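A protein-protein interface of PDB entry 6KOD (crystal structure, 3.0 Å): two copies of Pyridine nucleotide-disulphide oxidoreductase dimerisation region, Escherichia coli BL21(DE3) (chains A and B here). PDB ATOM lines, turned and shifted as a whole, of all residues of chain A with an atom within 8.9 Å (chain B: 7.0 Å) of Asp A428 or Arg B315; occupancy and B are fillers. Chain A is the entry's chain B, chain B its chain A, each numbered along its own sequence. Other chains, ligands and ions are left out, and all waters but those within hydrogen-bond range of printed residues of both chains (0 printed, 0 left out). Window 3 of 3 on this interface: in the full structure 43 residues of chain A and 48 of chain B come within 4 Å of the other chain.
The backbone carbonyl oxygen of Leu A426 lies close to the side-chain amide oxygen of Asn A441, 3.1 Å away.
O of Gln A429 sits close to OD1 of Asn A441 (2.9 Å).
The side-chain hydroxyl (OG) of Ser A445 sits at hydrogen-bond distance from the backbone carbonyl oxygen (O) of Asn A441 (3.0 Å).
NH2 of Arg B327 lies within salt-bridge range of OD1 of Asp B312 (2.9 Å).
NE of Arg B315 lies within salt-bridge range of OD2 of Asp B312, 3.2 Å away.
The guanidinium group (NH2) of Arg A427 lies within salt-bridge range of the side-chain carboxylate (OD2) of Asp A428 (2.6 Å).
Among the printed residues, pairs that only touch across the chains: Arg A427 with Arg B315, Asp A428 with Arg B315, Gln A429 with Arg B315, Gln A429 with Asp B418, Ile A430 with Tyr B308, Ile A430 with Ile B309, Ile A430 with Asp B312, Ile A430 with Arg B315, Phe A431 with Tyr B308 and Asn A441 with Leu B311.
Tyr A423 touches none of the printed residues of chain B.
Printed residues of chain B within 4 Å of Asn A441: Leu B311 (3.5 Å).
Printed residues of chain A within 4 Å of Tyr B308: Ile A430 and Phe A431.
Printed residues of chain A within 4 Å of Ile B309: Ile A430 (3.8 Å).
Of the printed residues of chain A, Asp B312 touches Ile A430.
Ile B316 touches none of the printed residues of chain A.
The nearest printed residue of chain A that does not touch Leu B311 is Gln A429 (5.2 Å).
Hydrophobic or aromatic side chains of chain B that line the printed part of chain A: Tyr B308, Ile B309 and Leu B311.
Along chain B the printed residues that touch a printed residue of chain A span positions 308 to 418.
Printed residues of chain A that touch a printed residue of chain B: Arg A427, Asp A428, Gln A429, Ile A430, Phe A431 and Asn A441.
Hydrophobic or aromatic side chains of chain A within 4 Å of the printed part of chain B: Ile A430.
Among the printed residues, no Asp or Glu carboxylate lies within 4 Å of a Lys or Arg side-chain nitrogen of the other chain.
No position is printed for both chains.
Of the 10 pairs that touch across the chains among the printed residues, none has its exchanged pair printed and touching as well.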
ATOM      1  N   GLN A 394      19.883  14.279  11.234  1.00  0.00           N
ATOM      2  CA  GLN A 394      20.426  14.862  10.008  1.00  0.00           C
ATOM      3  C   GLN A 394      21.870  14.450   9.734  1.00  0.00           C
ATOM      4  O   GLN A 394      22.477  14.950   8.779  1.00  0.00           O
ATOM      5  CB  GLN A 394      20.319  16.394  10.016  1.00  0.00           C
ATOM      6  CG  GLN A 394      18.905  16.924   9.831  1.00  0.00           C
ATOM      7  CD  GLN A 394      18.709  17.612   8.493  1.00  0.00           C
ATOM      8  OE1 GLN A 394      17.986  17.118   7.628  1.00  0.00           O
ATOM      9  NE2 GLN A 394      19.353  18.761   8.317  1.00  0.00           N
ATOM     10  N   PRO A 422      25.903  17.677  10.103  1.00  0.00           N
ATOM     11  CA  PRO A 422      24.866  17.027   9.295  1.00  0.00           C
ATOM     12  C   PRO A 422      25.324  16.836   7.858  1.00  0.00           C
ATOM     13  O   PRO A 422      26.368  17.330   7.427  1.00  0.00           O
ATOM     14  CB  PRO A 422      23.676  17.991   9.376  1.00  0.00           C
ATOM     15  CG  PRO A 422      24.042  19.011  10.420  1.00  0.00           C
ATOM     16  CD  PRO A 422      25.532  19.054  10.463  1.00  0.00           C
ATOM     17  N   TYR A 423      24.506  16.093   7.107  1.00  0.00           N
ATOM     18  CA  TYR A 423      24.807  15.845   5.701  1.00  0.00           C
ATOM     19  C   TYR A 423      24.842  17.136   4.896  1.00  0.00           C
ATOM     20  O   TYR A 423      25.503  17.200   3.854  1.00  0.00           O
ATOM     21  CB  TYR A 423      23.776  14.887   5.105  1.00  0.00           C
ATOM     22  CG  TYR A 423      22.448  15.544   4.807  1.00  0.00           C
ATOM     23  CD1 TYR A 423      21.511  15.743   5.811  1.00  0.00           C
ATOM     24  CD2 TYR A 423      22.133  15.970   3.523  1.00  0.00           C
ATOM     25  CE1 TYR A 423      20.296  16.347   5.547  1.00  0.00           C
ATOM     26  CE2 TYR A 423      20.923  16.578   3.249  1.00  0.00           C
ATOM     27  CZ  TYR A 423      20.007  16.762   4.264  1.00  0.00           C
ATOM     28  OH  TYR A 423      18.797  17.362   3.996  1.00  0.00           O
ATOM     29  N   SER A 424      24.135  18.171   5.361  1.00  0.00           N
ATOM     30  CA  SER A 424      24.072  19.429   4.625  1.00  0.00           C
ATOM     31  C   SER A 424      25.454  20.038   4.421  1.00  0.00           C
ATOM     32  O   SER A 424      25.666  20.776   3.452  1.00  0.00           O
ATOM     33  CB  SER A 424      23.166  20.418   5.358  1.00  0.00           C
ATOM     34  OG  SER A 424      23.883  21.111   6.365  1.00  0.00           O
ATOM     35  N   ILE A 425      26.398  19.743   5.318  1.00  0.00           N
ATOM     36  CA  ILE A 425      27.748  20.285   5.188  1.00  0.00           C
ATOM     37  C   ILE A 425      28.364  19.861   3.862  1.00  0.00           C
ATOM     38  O   ILE A 425      28.921  20.682   3.124  1.00  0.00           O
ATOM     39  CB  ILE A 425      28.618  19.849   6.381  1.00  0.00           C
ATOM     40  CG1 ILE A 425      28.197  20.594   7.650  1.00  0.00           C
ATOM     41  CG2 ILE A 425      30.092  20.085   6.086  1.00  0.00           C
ATOM     42  CD1 ILE A 425      28.670  22.032   7.702  1.00  0.00           C
ATOM     43  N   LEU A 426      28.258  18.572   3.532  1.00  0.00           N
ATOM     44  CA  LEU A 426      28.829  18.073   2.286  1.00  0.00           C
ATOM     45  C   LEU A 426      28.008  18.485   1.071  1.00  0.00           C
ATOM     46  O   LEU A 426      28.556  18.592  -0.032  1.00  0.00           O
ATOM     47  CB  LEU A 426      28.957  16.551   2.341  1.00  0.00           C
ATOM     48  CG  LEU A 426      30.091  16.029   3.223  1.00  0.00           C
ATOM     49  CD1 LEU A 426      30.083  14.507   3.250  1.00  0.00           C
ATOM     50  CD2 LEU A 426      31.435  16.567   2.744  1.00  0.00           C
ATOM     51  N   ARG A 427      26.705  18.716   1.249  1.00  0.00           N
ATOM     52  CA  ARG A 427      25.872  19.157   0.134  1.00  0.00           C
ATOM     53  C   ARG A 427      26.169  20.608  -0.230  1.00  0.00           C
ATOM     54  O   ARG A 427      26.448  20.923  -1.392  1.00  0.00           O
ATOM     55  CB  ARG A 427      24.394  18.976   0.481  1.00  0.00           C
ATOM     56  CG  ARG A 427      23.436  19.514  -0.570  1.00  0.00           C
ATOM     57  CD  ARG A 427      22.063  19.784   0.024  1.00  0.00           C
ATOM     58  NE  ARG A 427      22.102  20.832   1.041  1.00  0.00           N
ATOM     59  CZ  ARG A 427      21.213  20.953   2.021  1.00  0.00           C
ATOM     60  NH1 ARG A 427      20.212  20.090   2.116  1.00  0.00           N
ATOM     61  NH2 ARG A 427      21.325  21.934   2.907  1.00  0.00           N
ATOM     62  N   ASP A 428      26.112  21.506   0.755  1.00  0.00           N
ATOM     63  CA  ASP A 428      26.402  22.925   0.539  1.00  0.00           C
ATOM     64  C   ASP A 428      27.867  23.179   0.885  1.00  0.00           C
ATOM     65  O   ASP A 428      28.208  23.732   1.932  1.00  0.00           O
ATOM     66  CB  ASP A 428      25.473  23.800   1.372  1.00  0.00           C
ATOM     67  CG  ASP A 428      24.012  23.500   1.122  1.00  0.00           C
ATOM     68  OD1 ASP A 428      23.643  23.262  -0.046  1.00  0.00           O
ATOM     69  OD2 ASP A 428      23.230  23.505   2.097  1.00  0.00           O
ATOM     70  N   GLN A 429      28.748  22.760  -0.022  1.00  0.00           N
ATOM     71  CA  GLN A 429      30.184  22.904   0.178  1.00  0.00           C
ATOM     72  C   GLN A 429      30.853  23.248  -1.142  1.00  0.00           C
ATOM     73  O   GLN A 429      30.581  22.611  -2.164  1.00  0.00           O
ATOM     74  CB  GLN A 429      30.797  21.625   0.760  1.00  0.00           C
ATOM     75  CG  GLN A 429      32.315  21.635   0.820  1.00  0.00           C
ATOM     76  CD  GLN A 429      32.854  22.561   1.892  1.00  0.00           C
ATOM     77  OE1 GLN A 429      32.118  23.015   2.768  1.00  0.00           O
ATOM     78  NE2 GLN A 429      34.149  22.847   1.826  1.00  0.00           N
ATOM     79  N   ILE A 430      31.730  24.247  -1.114  1.00  0.00           N
ATOM     80  CA  ILE A 430      32.445  24.683  -2.309  1.00  0.00           C
ATOM     81  C   ILE A 430      33.650  23.768  -2.503  1.00  0.00           C
ATOM     82  O   ILE A 430      34.625  23.837  -1.753  1.00  0.00           O
ATOM     83  CB  ILE A 430      32.871  26.150  -2.204  1.00  0.00           C
ATOM     84  CG1 ILE A 430      31.638  27.058  -2.181  1.00  0.00           C
ATOM     85  CG2 ILE A 430      33.796  26.520  -3.354  1.00  0.00           C
ATOM     86  CD1 ILE A 430      31.935  28.505  -2.499  1.00  0.00           C
ATOM     87  N   PHE A 431      33.580  22.905  -3.511  1.00  0.00           N
ATOM     88  CA  PHE A 431      34.651  21.978  -3.831  1.00  0.00           C
ATOM     89  C   PHE A 431      35.436  22.485  -5.040  1.00  0.00           C
ATOM     90  O   PHE A 431      35.182  23.568  -5.572  1.00  0.00           O
ATOM     91  CB  PHE A 431      34.085  20.582  -4.090  1.00  0.00           C
ATOM     92  CG  PHE A 431      33.650  19.857  -2.849  1.00  0.00           C
ATOM     93  CD1 PHE A 431      34.582  19.428  -1.917  1.00  0.00           C
ATOM     94  CD2 PHE A 431      32.310  19.595  -2.618  1.00  0.00           C
ATOM     95  CE1 PHE A 431      34.185  18.755  -0.777  1.00  0.00           C
ATOM     96  CE2 PHE A 431      31.907  18.921  -1.480  1.00  0.00           C
ATOM     97  CZ  PHE A 431      32.846  18.500  -0.559  1.00  0.00           C
ATOM     98  N   GLU A 438      33.680  17.153  -5.426  1.00  0.00           N
ATOM     99  CA  GLU A 438      32.418  17.803  -5.757  1.00  0.00           C
ATOM    100  C   GLU A 438      31.329  16.808  -6.122  1.00  0.00           C
ATOM    101  O   GLU A 438      30.159  17.200  -6.211  1.00  0.00           O
ATOM    102  CB  GLU A 438      32.623  18.785  -6.909  1.00  0.00           C
ATOM    103  CG  GLU A 438      33.213  18.141  -8.144  1.00  0.00           C
ATOM    104  CD  GLU A 438      32.932  18.926  -9.403  1.00  0.00           C
ATOM    105  OE1 GLU A 438      32.025  19.785  -9.378  1.00  0.00           O
ATOM    106  OE2 GLU A 438      33.620  18.680 -10.417  1.00  0.00           O
ATOM    107  N   LEU A 440      30.260  14.794  -4.121  1.00  0.00           N
ATOM    108  CA  LEU A 440      29.438  14.804  -2.917  1.00  0.00           C
ATOM    109  C   LEU A 440      28.441  15.954  -2.906  1.00  0.00           C
ATOM    110  O   LEU A 440      27.462  15.898  -2.154  1.00  0.00           O
ATOM    111  CB  LEU A 440      30.326  14.873  -1.673  1.00  0.00           C
ATOM    112  CG  LEU A 440      31.179  13.631  -1.408  1.00  0.00           C
ATOM    113  CD1 LEU A 440      32.128  13.852  -0.235  1.00  0.00           C
ATOM    114  CD2 LEU A 440      30.288  12.422  -1.167  1.00  0.00           C
ATOM    115  N   ASN A 441      28.670  16.996  -3.710  1.00  0.00           N
ATOM    116  CA  ASN A 441      27.683  18.066  -3.830  1.00  0.00           C
ATOM    117  C   ASN A 441      26.379  17.539  -4.412  1.00  0.00           C
ATOM    118  O   ASN A 441      25.292  17.855  -3.911  1.00  0.00           O
ATOM    119  CB  ASN A 441      28.232  19.197  -4.702  1.00  0.00           C
ATOM    120  CG  ASN A 441      28.878  20.302  -3.892  1.00  0.00           C
ATOM    121  OD1 ASN A 441      28.942  20.234  -2.665  1.00  0.00           O
ATOM    122  ND2 ASN A 441      29.361  21.331  -4.579  1.00  0.00           N
ATOM    123  N   ASP A 442      26.468  16.722  -5.465  1.00  0.00           N
ATOM    124  CA  ASP A 442      25.278  16.196  -6.121  1.00  0.00           C
ATOM    125  C   ASP A 442      24.661  15.029  -5.359  1.00  0.00           C
ATOM    126  O   ASP A 442      23.452  14.798  -5.471  1.00  0.00           O
ATOM    127  CB  ASP A 442      25.615  15.760  -7.550  1.00  0.00           C
ATOM    128  CG  ASP A 442      26.175  16.894  -8.391  1.00  0.00           C
ATOM    129  OD1 ASP A 442      27.041  16.624  -9.251  1.00  0.00           O
ATOM    130  OD2 ASP A 442      25.752  18.052  -8.194  1.00  0.00           O
ATOM    131  N   PHE A 444      24.324  14.481  -1.992  1.00  0.00           N
ATOM    132  CA  PHE A 444      23.471  14.898  -0.891  1.00  0.00           C
ATOM    133  C   PHE A 444      22.451  15.948  -1.310  1.00  0.00           C
ATOM    134  O   PHE A 444      21.755  16.502  -0.454  1.00  0.00           O
ATOM    135  CB  PHE A 444      24.331  15.389   0.273  1.00  0.00           C
ATOM    136  CG  PHE A 444      25.184  14.309   0.877  1.00  0.00           C
ATOM    137  CD1 PHE A 444      24.609  13.293   1.624  1.00  0.00           C
ATOM    138  CD2 PHE A 444      26.553  14.288   0.670  1.00  0.00           C
ATOM    139  CE1 PHE A 444      25.387  12.288   2.172  1.00  0.00           C
ATOM    140  CE2 PHE A 444      27.336  13.285   1.216  1.00  0.00           C
ATOM    141  CZ  PHE A 444      26.751  12.283   1.964  1.00  0.00           C
ATOM    142  N   SER A 445      22.350  16.230  -2.610  1.00  0.00           N
ATOM    143  CA  SER A 445      21.211  16.965  -3.137  1.00  0.00           C
ATOM    144  C   SER A 445      20.012  16.059  -3.378  1.00  0.00           C
ATOM    145  O   SER A 445      18.877  16.546  -3.410  1.00  0.00           O
ATOM    146  CB  SER A 445      21.595  17.674  -4.436  1.00  0.00           C
ATOM    147  OG  SER A 445      22.433  18.786  -4.180  1.00  0.00           O
ATOM    148  N   ALA B  21      25.064  28.201 -12.754  1.00  0.00           N
ATOM    149  CA  ALA B  21      24.066  28.710 -11.820  1.00  0.00           C
ATOM    150  C   ALA B  21      22.673  28.679 -12.434  1.00  0.00           C
ATOM    151  O   ALA B  21      21.723  28.177 -11.821  1.00  0.00           O
ATOM    152  CB  ALA B  21      24.428  30.127 -11.386  1.00  0.00           C
ATOM    153  N   MET B 297      24.097  35.800 -11.609  1.00  0.00           N
ATOM    154  CA  MET B 297      24.981  34.787 -11.054  1.00  0.00           C
ATOM    155  C   MET B 297      26.029  34.380 -12.084  1.00  0.00           C
ATOM    156  O   MET B 297      25.808  34.481 -13.294  1.00  0.00           O
ATOM    157  CB  MET B 297      24.204  33.544 -10.605  1.00  0.00           C
ATOM    158  CG  MET B 297      22.951  33.827  -9.808  1.00  0.00           C
ATOM    159  SD  MET B 297      21.477  33.750 -10.832  1.00  0.00           S
ATOM    160  CE  MET B 297      21.382  31.997 -11.168  1.00  0.00           C
ATOM    161  N   TYR B 308      32.607  26.332  -9.572  1.00  0.00           N
ATOM    162  CA  TYR B 308      32.082  26.084  -8.234  1.00  0.00           C
ATOM    163  C   TYR B 308      31.658  27.360  -7.519  1.00  0.00           C
ATOM    164  O   TYR B 308      30.953  27.275  -6.508  1.00  0.00           O
ATOM    165  CB  TYR B 308      33.102  25.318  -7.380  1.00  0.00           C
ATOM    166  CG  TYR B 308      34.537  25.800  -7.463  1.00  0.00           C
ATOM    167  CD1 TYR B 308      35.426  25.246  -8.377  1.00  0.00           C
ATOM    168  CD2 TYR B 308      35.014  26.783  -6.604  1.00  0.00           C
ATOM    169  CE1 TYR B 308      36.742  25.673  -8.447  1.00  0.00           C
ATOM    170  CE2 TYR B 308      36.328  27.216  -6.667  1.00  0.00           C
ATOM    171  CZ  TYR B 308      37.188  26.658  -7.590  1.00  0.00           C
ATOM    172  OH  TYR B 308      38.494  27.086  -7.656  1.00  0.00           O
ATOM    173  N   ILE B 309      32.058  28.533  -8.013  1.00  0.00           N
ATOM    174  CA  ILE B 309      31.546  29.781  -7.457  1.00  0.00           C
ATOM    175  C   ILE B 309      30.153  30.074  -8.001  1.00  0.00           C
ATOM    176  O   ILE B 309      29.262  30.508  -7.262  1.00  0.00           O
ATOM    177  CB  ILE B 309      32.523  30.936  -7.741  1.00  0.00           C
ATOM    178  CG1 ILE B 309      33.726  30.864  -6.800  1.00  0.00           C
ATOM    179  CG2 ILE B 309      31.827  32.280  -7.595  1.00  0.00           C
ATOM    180  CD1 ILE B 309      33.367  30.518  -5.371  1.00  0.00           C
ATOM    181  N   SER B 310      29.943  29.831  -9.298  1.00  0.00           N
ATOM    182  CA  SER B 310      28.628  30.043  -9.893  1.00  0.00           C
ATOM    183  C   SER B 310      27.572  29.171  -9.225  1.00  0.00           C
ATOM    184  O   SER B 310      26.441  29.616  -9.000  1.00  0.00           O
ATOM    185  CB  SER B 310      28.692  29.768 -11.397  1.00  0.00           C
ATOM    186  OG  SER B 310      27.426  29.408 -11.917  1.00  0.00           O
ATOM    187  N   LEU B 311      27.927  27.927  -8.891  1.00  0.00           N
ATOM    188  CA  LEU B 311      26.999  27.067  -8.161  1.00  0.00           C
ATOM    189  C   LEU B 311      26.671  27.656  -6.796  1.00  0.00           C
ATOM    190  O   LEU B 311      25.538  27.534  -6.313  1.00  0.00           O
ATOM    191  CB  LEU B 311      27.589  25.663  -8.014  1.00  0.00           C
ATOM    192  CG  LEU B 311      26.778  24.653  -7.197  1.00  0.00           C
ATOM    193  CD1 LEU B 311      25.904  23.805  -8.102  1.00  0.00           C
ATOM    194  CD2 LEU B 311      27.698  23.776  -6.365  1.00  0.00           C
ATOM    195  N   ASP B 312      27.650  28.297  -6.156  1.00  0.00           N
ATOM    196  CA  ASP B 312      27.381  28.952  -4.882  1.00  0.00           C
ATOM    197  C   ASP B 312      26.553  30.214  -5.080  1.00  0.00           C
ATOM    198  O   ASP B 312      25.711  30.550  -4.237  1.00  0.00           O
ATOM    199  CB  ASP B 312      28.687  29.275  -4.168  1.00  0.00           C
ATOM    200  CG  ASP B 312      28.501  29.415  -2.682  1.00  0.00           C
ATOM    201  OD1 ASP B 312      28.993  30.405  -2.106  1.00  0.00           O
ATOM    202  OD2 ASP B 312      27.839  28.537  -2.087  1.00  0.00           O
ATOM    203  N   ASP B 313      26.789  30.933  -6.180  1.00  0.00           N
ATOM    204  CA  ASP B 313      25.890  32.014  -6.561  1.00  0.00           C
ATOM    205  C   ASP B 313      24.461  31.502  -6.689  1.00  0.00           C
ATOM    206  O   ASP B 313      23.513  32.157  -6.236  1.00  0.00           O
ATOM    207  CB  ASP B 313      26.359  32.640  -7.877  1.00  0.00           C
ATOM    208  CG  ASP B 313      27.386  33.741  -7.674  1.00  0.00           C
ATOM    209  OD1 ASP B 313      27.482  34.271  -6.547  1.00  0.00           O
ATOM    210  OD2 ASP B 313      28.089  34.085  -8.648  1.00  0.00           O
ATOM    211  N   TYR B 314      24.292  30.324  -7.293  1.00  0.00           N
ATOM    212  CA  TYR B 314      22.976  29.700  -7.380  1.00  0.00           C
ATOM    213  C   TYR B 314      22.377  29.487  -5.994  1.00  0.00           C
ATOM    214  O   TYR B 314      21.213  29.822  -5.750  1.00  0.00           O
ATOM    215  CB  TYR B 314      23.085  28.373  -8.137  1.00  0.00           C
ATOM    216  CG  TYR B 314      22.090  27.318  -7.705  1.00  0.00           C
ATOM    217  CD1 TYR B 314      20.721  27.530  -7.818  1.00  0.00           C
ATOM    218  CD2 TYR B 314      22.523  26.113  -7.167  1.00  0.00           C
ATOM    219  CE1 TYR B 314      19.816  26.573  -7.414  1.00  0.00           C
ATOM    220  CE2 TYR B 314      21.623  25.149  -6.760  1.00  0.00           C
ATOM    221  CZ  TYR B 314      20.272  25.384  -6.888  1.00  0.00           C
ATOM    222  OH  TYR B 314      19.365  24.430  -6.486  1.00  0.00           O
ATOM    223  N   ARG B 315      23.161  28.922  -5.072  1.00  0.00           N
ATOM    224  CA  ARG B 315      22.653  28.651  -3.732  1.00  0.00           C
ATOM    225  C   ARG B 315      22.221  29.927  -3.024  1.00  0.00           C
ATOM    226  O   ARG B 315      21.252  29.912  -2.255  1.00  0.00           O
ATOM    227  CB  ARG B 315      23.712  27.918  -2.908  1.00  0.00           C
ATOM    228  CG  ARG B 315      23.955  26.484  -3.344  1.00  0.00           C
ATOM    229  CD  ARG B 315      24.669  25.694  -2.260  1.00  0.00           C
ATOM    230  NE  ARG B 315      26.115  25.892  -2.306  1.00  0.00           N
ATOM    231  CZ  ARG B 315      26.974  25.009  -2.804  1.00  0.00           C
ATOM    232  NH1 ARG B 315      26.532  23.860  -3.297  1.00  0.00           N
ATOM    233  NH2 ARG B 315      28.273  25.270  -2.809  1.00  0.00           N
ATOM    234  N   ILE B 316      22.918  31.038  -3.274  1.00  0.00           N
ATOM    235  CA  ILE B 316      22.550  32.307  -2.655  1.00  0.00           C
ATOM    236  C   ILE B 316      21.197  32.783  -3.171  1.00  0.00           C
ATOM    237  O   ILE B 316      20.347  33.242  -2.399  1.00  0.00           O
ATOM    238  CB  ILE B 316      23.656  33.350  -2.899  1.00  0.00           C
ATOM    239  CG1 ILE B 316      24.900  33.005  -2.079  1.00  0.00           C
ATOM    240  CG2 ILE B 316      23.163  34.749  -2.573  1.00  0.00           C
ATOM    241  CD1 ILE B 316      26.188  33.486  -2.701  1.00  0.00           C
ATOM    242  N   VAL B 317      20.972  32.671  -4.481  1.00  0.00           N
ATOM    243  CA  VAL B 317      19.698  33.087  -5.058  1.00  0.00           C
ATOM    244  C   VAL B 317      18.585  32.126  -4.652  1.00  0.00           C
ATOM    245  O   VAL B 317      17.445  32.542  -4.410  1.00  0.00           O
ATOM    246  CB  VAL B 317      19.833  33.207  -6.587  1.00  0.00           C
ATOM    247  CG1 VAL B 317      18.470  33.334  -7.251  1.00  0.00           C
ATOM    248  CG2 VAL B 317      20.718  34.392  -6.943  1.00  0.00           C
ATOM    249  N   ARG B 318      18.894  30.829  -4.559  1.00  0.00           N
ATOM    250  CA  ARG B 318      17.892  29.862  -4.119  1.00  0.00           C
ATOM    251  C   ARG B 318      17.491  30.102  -2.667  1.00  0.00           C
ATOM    252  O   ARG B 318      16.316  29.960  -2.310  1.00  0.00           O
ATOM    253  CB  ARG B 318      18.417  28.438  -4.302  1.00  0.00           C
ATOM    254  CG  ARG B 318      17.342  27.362  -4.220  1.00  0.00           C
ATOM    255  CD  ARG B 318      17.723  26.263  -3.236  1.00  0.00           C
ATOM    256  NE  ARG B 318      17.242  26.544  -1.885  1.00  0.00           N
ATOM    257  CZ  ARG B 318      16.064  26.148  -1.414  1.00  0.00           C
ATOM    258  NH1 ARG B 318      15.707  26.450  -0.173  1.00  0.00           N
ATOM    259  NH2 ARG B 318      15.240  25.448  -2.183  1.00  0.00           N
ATOM    260  N   ASP B 319      18.455  30.462  -1.815  1.00  0.00           N
ATOM    261  CA  ASP B 319      18.144  30.786  -0.427  1.00  0.00           C
ATOM    262  C   ASP B 319      17.345  32.077  -0.303  1.00  0.00           C
ATOM    263  O   ASP B 319      16.705  32.301   0.729  1.00  0.00           O
ATOM    264  CB  ASP B 319      19.437  30.890   0.387  1.00  0.00           C
ATOM    265  CG  ASP B 319      19.197  30.809   1.884  1.00  0.00           C
ATOM    266  OD1 ASP B 319      19.067  31.874   2.525  1.00  0.00           O
ATOM    267  OD2 ASP B 319      19.139  29.682   2.419  1.00  0.00           O
ATOM    268  N   GLU B 320      17.369  32.925  -1.328  1.00  0.00           N
ATOM    269  CA  GLU B 320      16.607  34.167  -1.323  1.00  0.00           C
ATOM    270  C   GLU B 320      15.180  33.958  -1.817  1.00  0.00           C
ATOM    271  O   GLU B 320      14.229  34.457  -1.208  1.00  0.00           O
ATOM    272  CB  GLU B 320      17.315  35.214  -2.188  1.00  0.00           C
ATOM    273  CG  GLU B 320      16.538  36.502  -2.353  1.00  0.00           C
ATOM    274  CD  GLU B 320      16.779  37.465  -1.214  1.00  0.00           C
ATOM    275  OE1 GLU B 320      17.940  37.564  -0.763  1.00  0.00           O
ATOM    276  OE2 GLU B 320      15.812  38.121  -0.772  1.00  0.00           O
ATOM    277  N   ARG B 327      21.157  34.321   2.621  1.00  0.00           N
ATOM    278  CA  ARG B 327      22.555  33.943   2.745  1.00  0.00           C
ATOM    279  C   ARG B 327      23.357  34.706   1.699  1.00  0.00           C
ATOM    280  O   ARG B 327      22.921  34.842   0.553  1.00  0.00           O
ATOM    281  CB  ARG B 327      22.717  32.429   2.581  1.00  0.00           C
ATOM    282  CG  ARG B 327      23.807  31.981   1.633  1.00  0.00           C
ATOM    283  CD  ARG B 327      23.982  30.477   1.741  1.00  0.00           C
ATOM    284  NE  ARG B 327      24.886  29.939   0.732  1.00  0.00           N
ATOM    285  CZ  ARG B 327      26.202  30.116   0.734  1.00  0.00           C
ATOM    286  NH1 ARG B 327      26.785  30.822   1.692  1.00  0.00           N
ATOM    287  NH2 ARG B 327      26.938  29.579  -0.222  1.00  0.00           N
ATOM    288  N   ASP B 418      37.440  25.832   7.160  1.00  0.00           N
ATOM    289  CA  ASP B 418      36.058  26.305   7.140  1.00  0.00           C
ATOM    290  C   ASP B 418      35.411  26.126   8.505  1.00  0.00           C
ATOM    291  O   ASP B 418      34.996  27.098   9.147  1.00  0.00           O
ATOM    292  CB  ASP B 418      35.263  25.562   6.066  1.00  0.00           C
ATOM    293  CG  ASP B 418      35.152  26.348   4.779  1.00  0.00           C
ATOM    294  OD1 ASP B 418      35.652  27.493   4.734  1.00  0.00           O
ATOM    295  OD2 ASP B 418      34.566  25.821   3.810  1.00  0.00           O
